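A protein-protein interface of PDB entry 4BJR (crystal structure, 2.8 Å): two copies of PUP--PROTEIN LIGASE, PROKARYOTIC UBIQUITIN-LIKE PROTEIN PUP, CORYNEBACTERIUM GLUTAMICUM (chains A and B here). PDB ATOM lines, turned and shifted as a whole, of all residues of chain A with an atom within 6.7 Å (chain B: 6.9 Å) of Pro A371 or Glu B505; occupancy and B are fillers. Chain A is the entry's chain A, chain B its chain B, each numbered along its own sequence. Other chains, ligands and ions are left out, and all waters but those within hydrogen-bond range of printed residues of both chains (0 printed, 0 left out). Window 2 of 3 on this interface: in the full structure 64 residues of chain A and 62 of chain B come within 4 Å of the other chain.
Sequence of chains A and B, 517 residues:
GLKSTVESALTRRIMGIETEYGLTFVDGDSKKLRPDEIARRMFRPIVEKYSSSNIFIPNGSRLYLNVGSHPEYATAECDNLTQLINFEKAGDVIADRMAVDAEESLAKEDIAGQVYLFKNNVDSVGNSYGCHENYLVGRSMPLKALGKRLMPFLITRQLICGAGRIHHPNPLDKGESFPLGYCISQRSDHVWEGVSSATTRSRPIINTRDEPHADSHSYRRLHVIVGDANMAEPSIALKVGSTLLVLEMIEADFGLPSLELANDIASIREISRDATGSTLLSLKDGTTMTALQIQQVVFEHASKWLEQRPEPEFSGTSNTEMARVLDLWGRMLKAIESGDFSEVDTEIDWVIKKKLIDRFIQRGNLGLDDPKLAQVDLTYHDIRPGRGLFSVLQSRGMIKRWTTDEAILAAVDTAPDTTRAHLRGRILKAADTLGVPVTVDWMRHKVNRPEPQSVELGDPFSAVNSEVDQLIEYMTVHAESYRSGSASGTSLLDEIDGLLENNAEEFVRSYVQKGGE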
ATOM      1  N   GLY A 367     -10.631  16.334  -9.262  1.00  0.00           N
ATOM      2  CA  GLY A 367     -10.844  15.987  -7.874  1.00  0.00           C
ATOM      3  C   GLY A 367     -11.024  14.490  -7.757  1.00  0.00           C
ATOM      4  O   GLY A 367     -11.221  13.817  -8.756  1.00  0.00           O
ATOM      5  N   LEU A 368     -10.924  13.963  -6.545  1.00  0.00           N
ATOM      6  CA  LEU A 368     -11.152  12.543  -6.314  1.00  0.00           C
ATOM      7  C   LEU A 368     -12.587  12.129  -6.574  1.00  0.00           C
ATOM      8  O   LEU A 368     -12.858  11.001  -6.961  1.00  0.00           O
ATOM      9  CB  LEU A 368     -10.783  12.170  -4.889  1.00  0.00           C
ATOM     10  CG  LEU A 368     -10.116  10.810  -4.742  1.00  0.00           C
ATOM     11  CD1 LEU A 368      -8.890  10.733  -5.621  1.00  0.00           C
ATOM     12  CD2 LEU A 368      -9.755  10.591  -3.307  1.00  0.00           C
ATOM     13  N   ASP A 369     -13.509  13.042  -6.322  1.00  0.00           N
ATOM     14  CA  ASP A 369     -14.918  12.773  -6.529  1.00  0.00           C
ATOM     15  C   ASP A 369     -15.291  12.706  -8.004  1.00  0.00           C
ATOM     16  O   ASP A 369     -16.424  12.389  -8.342  1.00  0.00           O
ATOM     17  CB  ASP A 369     -15.750  13.829  -5.813  1.00  0.00           C
ATOM     18  CG  ASP A 369     -15.153  15.208  -5.929  1.00  0.00           C
ATOM     19  OD1 ASP A 369     -14.057  15.330  -6.504  1.00  0.00           O
ATOM     20  OD2 ASP A 369     -15.763  16.170  -5.428  1.00  0.00           O
ATOM     21  N   ASP A 370     -14.342  13.023  -8.876  1.00  0.00           N
ATOM     22  CA  ASP A 370     -14.585  13.027 -10.311  1.00  0.00           C
ATOM     23  C   ASP A 370     -14.998  11.638 -10.796  1.00  0.00           C
ATOM     24  O   ASP A 370     -14.367  10.646 -10.452  1.00  0.00           O
ATOM     25  CB  ASP A 370     -13.340  13.498 -11.048  1.00  0.00           C
ATOM     26  CG  ASP A 370     -13.579  13.710 -12.511  1.00  0.00           C
ATOM     27  OD1 ASP A 370     -13.652  12.722 -13.254  1.00  0.00           O
ATOM     28  OD2 ASP A 370     -13.694  14.880 -12.922  1.00  0.00           O
ATOM     29  N   PRO A 371     -16.062  11.569 -11.603  1.00  0.00           N
ATOM     30  CA  PRO A 371     -16.661  10.320 -12.072  1.00  0.00           C
ATOM     31  C   PRO A 371     -15.725   9.470 -12.903  1.00  0.00           C
ATOM     32  O   PRO A 371     -15.788   8.247 -12.850  1.00  0.00           O
ATOM     33  CB  PRO A 371     -17.826  10.808 -12.923  1.00  0.00           C
ATOM     34  CG  PRO A 371     -18.176  12.103 -12.340  1.00  0.00           C
ATOM     35  CD  PRO A 371     -16.856  12.724 -12.039  1.00  0.00           C
ATOM     36  N   LYS A 372     -14.882  10.122 -13.682  1.00  0.00           N
ATOM     37  CA  LYS A 372     -13.964   9.431 -14.559  1.00  0.00           C
ATOM     38  C   LYS A 372     -13.064   8.517 -13.734  1.00  0.00           C
ATOM     39  O   LYS A 372     -12.755   7.396 -14.129  1.00  0.00           O
ATOM     40  CB  LYS A 372     -13.147  10.445 -15.352  1.00  0.00           C
ATOM     41  CG  LYS A 372     -12.261   9.864 -16.420  1.00  0.00           C
ATOM     42  CD  LYS A 372     -13.032   9.661 -17.699  1.00  0.00           C
ATOM     43  CE  LYS A 372     -12.109   9.393 -18.868  1.00  0.00           C
ATOM     44  NZ  LYS A 372     -11.680  10.629 -19.575  1.00  0.00           N
ATOM     45  N   LEU A 373     -12.669   9.003 -12.568  1.00  0.00           N
ATOM     46  CA  LEU A 373     -11.818   8.253 -11.666  1.00  0.00           C
ATOM     47  C   LEU A 373     -12.505   7.020 -11.134  1.00  0.00           C
ATOM     48  O   LEU A 373     -11.904   5.962 -11.063  1.00  0.00           O
ATOM     49  CB  LEU A 373     -11.385   9.136 -10.512  1.00  0.00           C
ATOM     50  CG  LEU A 373     -10.514  10.311 -10.922  1.00  0.00           C
ATOM     51  CD1 LEU A 373     -10.007  11.005  -9.695  1.00  0.00           C
ATOM     52  CD2 LEU A 373      -9.369   9.835 -11.771  1.00  0.00           C
ATOM     53  N   ALA A 374     -13.762   7.163 -10.745  1.00  0.00           N
ATOM     54  CA  ALA A 374     -14.554   6.033 -10.283  1.00  0.00           C
ATOM     55  C   ALA A 374     -14.706   5.001 -11.384  1.00  0.00           C
ATOM     56  O   ALA A 374     -14.661   3.794 -11.143  1.00  0.00           O
ATOM     57  CB  ALA A 374     -15.900   6.498  -9.812  1.00  0.00           C
ATOM     58  N   GLN A 375     -14.870   5.494 -12.603  1.00  0.00           N
ATOM     59  CA  GLN A 375     -14.963   4.637 -13.763  1.00  0.00           C
ATOM     60  C   GLN A 375     -13.681   3.853 -13.958  1.00  0.00           C
ATOM     61  O   GLN A 375     -13.713   2.677 -14.290  1.00  0.00           O
ATOM     62  CB  GLN A 375     -15.280   5.457 -15.004  1.00  0.00           C
ATOM     63  CG  GLN A 375     -15.638   4.612 -16.191  1.00  0.00           C
ATOM     64  CD  GLN A 375     -15.865   5.417 -17.441  1.00  0.00           C
ATOM     65  OE1 GLN A 375     -15.383   6.535 -17.570  1.00  0.00           O
ATOM     66  NE2 GLN A 375     -16.598   4.845 -18.379  1.00  0.00           N
ATOM     67  N   VAL A 376     -12.548   4.505 -13.753  1.00  0.00           N
ATOM     68  CA  VAL A 376     -11.265   3.825 -13.832  1.00  0.00           C
ATOM     69  C   VAL A 376     -11.118   2.771 -12.744  1.00  0.00           C
ATOM     70  O   VAL A 376     -10.651   1.655 -12.986  1.00  0.00           O
ATOM     71  CB  VAL A 376     -10.123   4.825 -13.722  1.00  0.00           C
ATOM     72  CG1 VAL A 376      -8.810   4.114 -13.580  1.00  0.00           C
ATOM     73  CG2 VAL A 376     -10.117   5.731 -14.922  1.00  0.00           C
ATOM     74  N   GLU B 501     -16.672   4.216 -21.628  1.00  0.00           N
ATOM     75  CA  GLU B 501     -17.952   4.818 -21.954  1.00  0.00           C
ATOM     76  C   GLU B 501     -17.906   6.276 -21.582  1.00  0.00           C
ATOM     77  O   GLU B 501     -17.485   6.632 -20.490  1.00  0.00           O
ATOM     78  CB  GLU B 501     -19.093   4.123 -21.224  1.00  0.00           C
ATOM     79  CG  GLU B 501     -19.198   2.650 -21.509  1.00  0.00           C
ATOM     80  CD  GLU B 501     -19.792   2.380 -22.866  1.00  0.00           C
ATOM     81  OE1 GLU B 501     -19.033   2.350 -23.852  1.00  0.00           O
ATOM     82  OE2 GLU B 501     -21.023   2.214 -22.949  1.00  0.00           O
ATOM     83  N   ASN B 502     -18.364   7.120 -22.490  1.00  0.00           N
ATOM     84  CA  ASN B 502     -18.200   8.551 -22.346  1.00  0.00           C
ATOM     85  C   ASN B 502     -18.920   9.129 -21.153  1.00  0.00           C
ATOM     86  O   ASN B 502     -18.406  10.026 -20.496  1.00  0.00           O
ATOM     87  CB  ASN B 502     -18.640   9.251 -23.615  1.00  0.00           C
ATOM     88  CG  ASN B 502     -17.536   9.315 -24.631  1.00  0.00           C
ATOM     89  OD1 ASN B 502     -16.547   8.594 -24.528  1.00  0.00           O
ATOM     90  ND2 ASN B 502     -17.682  10.190 -25.612  1.00  0.00           N
ATOM     91  N   ASN B 503     -20.106   8.630 -20.854  1.00  0.00           N
ATOM     92  CA  ASN B 503     -20.749   9.111 -19.657  1.00  0.00           C
ATOM     93  C   ASN B 503     -20.309   8.231 -18.518  1.00  0.00           C
ATOM     94  O   ASN B 503     -20.874   7.169 -18.286  1.00  0.00           O
ATOM     95  CB  ASN B 503     -22.259   9.079 -19.815  1.00  0.00           C
ATOM     96  CG  ASN B 503     -22.972   9.751 -18.674  1.00  0.00           C
ATOM     97  OD1 ASN B 503     -22.446   9.856 -17.567  1.00  0.00           O
ATOM     98  ND2 ASN B 503     -24.187  10.206 -18.930  1.00  0.00           N
ATOM     99  N   ALA B 504     -19.344   8.732 -17.759  1.00  0.00           N
ATOM    100  CA  ALA B 504     -18.745   7.980 -16.676  1.00  0.00           C
ATOM    101  C   ALA B 504     -19.647   7.916 -15.478  1.00  0.00           C
ATOM    102  O   ALA B 504     -19.801   6.870 -14.865  1.00  0.00           O
ATOM    103  CB  ALA B 504     -17.430   8.585 -16.300  1.00  0.00           C
ATOM    104  N   GLU B 505     -20.236   9.046 -15.138  1.00  0.00           N
ATOM    105  CA  GLU B 505     -21.038   9.098 -13.942  1.00  0.00           C
ATOM    106  C   GLU B 505     -22.219   8.171 -14.057  1.00  0.00           C
ATOM    107  O   GLU B 505     -22.545   7.471 -13.118  1.00  0.00           O
ATOM    108  CB  GLU B 505     -21.534  10.509 -13.656  1.00  0.00           C
ATOM    109  CG  GLU B 505     -22.215  10.611 -12.297  1.00  0.00           C
ATOM    110  CD  GLU B 505     -23.154  11.784 -12.188  1.00  0.00           C
ATOM    111  OE1 GLU B 505     -22.836  12.852 -12.744  1.00  0.00           O
ATOM    112  OE2 GLU B 505     -24.208  11.640 -11.538  1.00  0.00           O
ATOM    113  N   GLU B 506     -22.851   8.160 -15.217  1.00  0.00           N
ATOM    114  CA  GLU B 506     -23.992   7.296 -15.414  1.00  0.00           C
ATOM    115  C   GLU B 506     -23.574   5.841 -15.425  1.00  0.00           C
ATOM    116  O   GLU B 506     -24.293   4.983 -14.940  1.00  0.00           O
ATOM    117  CB  GLU B 506     -24.719   7.649 -16.700  1.00  0.00           C
ATOM    118  CG  GLU B 506     -26.207   7.423 -16.594  1.00  0.00           C
ATOM    119  CD  GLU B 506     -26.821   8.175 -15.423  1.00  0.00           C
ATOM    120  OE1 GLU B 506     -26.338   9.278 -15.094  1.00  0.00           O
ATOM    121  OE2 GLU B 506     -27.779   7.656 -14.817  1.00  0.00           O
ATOM    122  N   PHE B 507     -22.409   5.570 -15.990  1.00  0.00           N
ATOM    123  CA  PHE B 507     -21.887   4.216 -16.067  1.00  0.00           C
ATOM    124  C   PHE B 507     -21.656   3.650 -14.677  1.00  0.00           C
ATOM    125  O   PHE B 507     -22.052   2.534 -14.379  1.00  0.00           O
ATOM    126  CB  PHE B 507     -20.593   4.204 -16.864  1.00  0.00           C
ATOM    127  CG  PHE B 507     -20.019   2.846 -17.078  1.00  0.00           C
ATOM    128  CD1 PHE B 507     -20.588   1.979 -17.971  1.00  0.00           C
ATOM    129  CD2 PHE B 507     -18.895   2.447 -16.407  1.00  0.00           C
ATOM    130  CE1 PHE B 507     -20.048   0.736 -18.179  1.00  0.00           C
ATOM    131  CE2 PHE B 507     -18.360   1.208 -16.614  1.00  0.00           C
ATOM    132  CZ  PHE B 507     -18.937   0.354 -17.498  1.00  0.00           C
ATOM    133  N   VAL B 508     -21.017   4.437 -13.826  1.00  0.00           N
ATOM    134  CA  VAL B 508     -20.761   4.044 -12.454  1.00  0.00           C
ATOM    135  C   VAL B 508     -22.029   3.951 -11.633  1.00  0.00           C
ATOM    136  O   VAL B 508     -22.227   3.014 -10.877  1.00  0.00           O
ATOM    137  CB  VAL B 508     -19.811   5.037 -11.780  1.00  0.00           C
ATOM    138  CG1 VAL B 508     -19.693   4.753 -10.304  1.00  0.00           C
ATOM    139  CG2 VAL B 508     -18.461   4.983 -12.436  1.00  0.00           C
ATOM    140  N   ARG B 509     -22.894   4.936 -11.801  1.00  0.00           N
ATOM    141  CA  ARG B 509     -24.135   5.016 -11.055  1.00  0.00           C
ATOM    142  C   ARG B 509     -24.996   3.808 -11.351  1.00  0.00           C
ATOM    143  O   ARG B 509     -25.667   3.272 -10.476  1.00  0.00           O
ATOM    144  CB  ARG B 509     -24.869   6.302 -11.398  1.00  0.00           C
ATOM    145  CG  ARG B 509     -26.122   6.521 -10.618  1.00  0.00           C
ATOM    146  CD  ARG B 509     -26.789   7.813 -11.008  1.00  0.00           C
ATOM    147  NE  ARG B 509     -28.062   7.965 -10.321  1.00  0.00           N
ATOM    148  CZ  ARG B 509     -28.793   9.070 -10.341  1.00  0.00           C
ATOM    149  NH1 ARG B 509     -28.375  10.130 -11.014  1.00  0.00           N
ATOM    150  NH2 ARG B 509     -29.943   9.113  -9.683  1.00  0.00           N
ATOM    151  N   SER B 510     -24.974   3.400 -12.610  1.00  0.00           N
ATOM    152  CA  SER B 510     -25.752   2.273 -13.089  1.00  0.00           C
ATOM    153  C   SER B 510     -25.357   0.946 -12.465  1.00  0.00           C
ATOM    154  O   SER B 510     -26.201   0.085 -12.256  1.00  0.00           O
ATOM    155  CB  SER B 510     -25.631   2.164 -14.600  1.00  0.00           C
ATOM    156  OG  SER B 510     -26.094   0.906 -15.039  1.00  0.00           O
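O of Glu B501 lies within hydrogen-bond range of NE2 of Gln A375.
The backbone NH (N) of Glu B505 lies within hydrogen-bond range of the side-chain amide oxygen (OD1) of Asn B503 (3.4 Å). The backbone NH of Lys A372 is in hydrogen-bond range of the side-chain carboxylate of Asp A370.
Among the printed residues, pairs that only touch across the chains: Pro A371 with Ala B504, Pro A371 with Glu B505, Lys A372 with Ala B504, Ala A374 with Val B508, Gln A375 with Ala B504, Gln A375 with Phe B507 and Gln A375 with Val B508.
Of the printed residues of chain B, Pro A371 touches Ala B504 (3.8 Å) and Glu B505 (3.7 Å). Glu B505 touches one residue of chain A. Printed residues of chain B within 4 Å of Ala A374: Val B508 (3.9 Å). Printed residues of chain B within 4 Å of Gln A375: Glu B501, Ala B504, Phe B507 and Val B508. The nearest residue of chain B that does not touch Pro A371 is Val B508 (4.2 Å). The nearest residue of chain A that does not touch Glu B505 is Lys A372 (5.7 Å).
Printed residues of chain B that touch a printed residue of chain A: Glu B501, Ala B504, Glu B505, Phe B507 and Val B508. Hydrophobic or aromatic side chains of chain B that line the printed part of chain A: Ala B504, Phe B507 and Val B508. Along chain B the printed residues that touch a printed residue of chain A span positions 501 to 508. Of the 10 printed residues of chain A, 4 touch a printed residue of chain B. Hydrophobic or aromatic side chains of chain A that line the printed part of chain B: Pro A371 and Ala A374. Among the printed residues, no Asp or Glu carboxylate lies within 4 Å of a Lys or Arg side-chain nitrogen of the other chain.
No position is printed for both chains. Of the 8 pairs that touch across the chains among the printed residues, none has its exchanged pair printed and touching as well.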
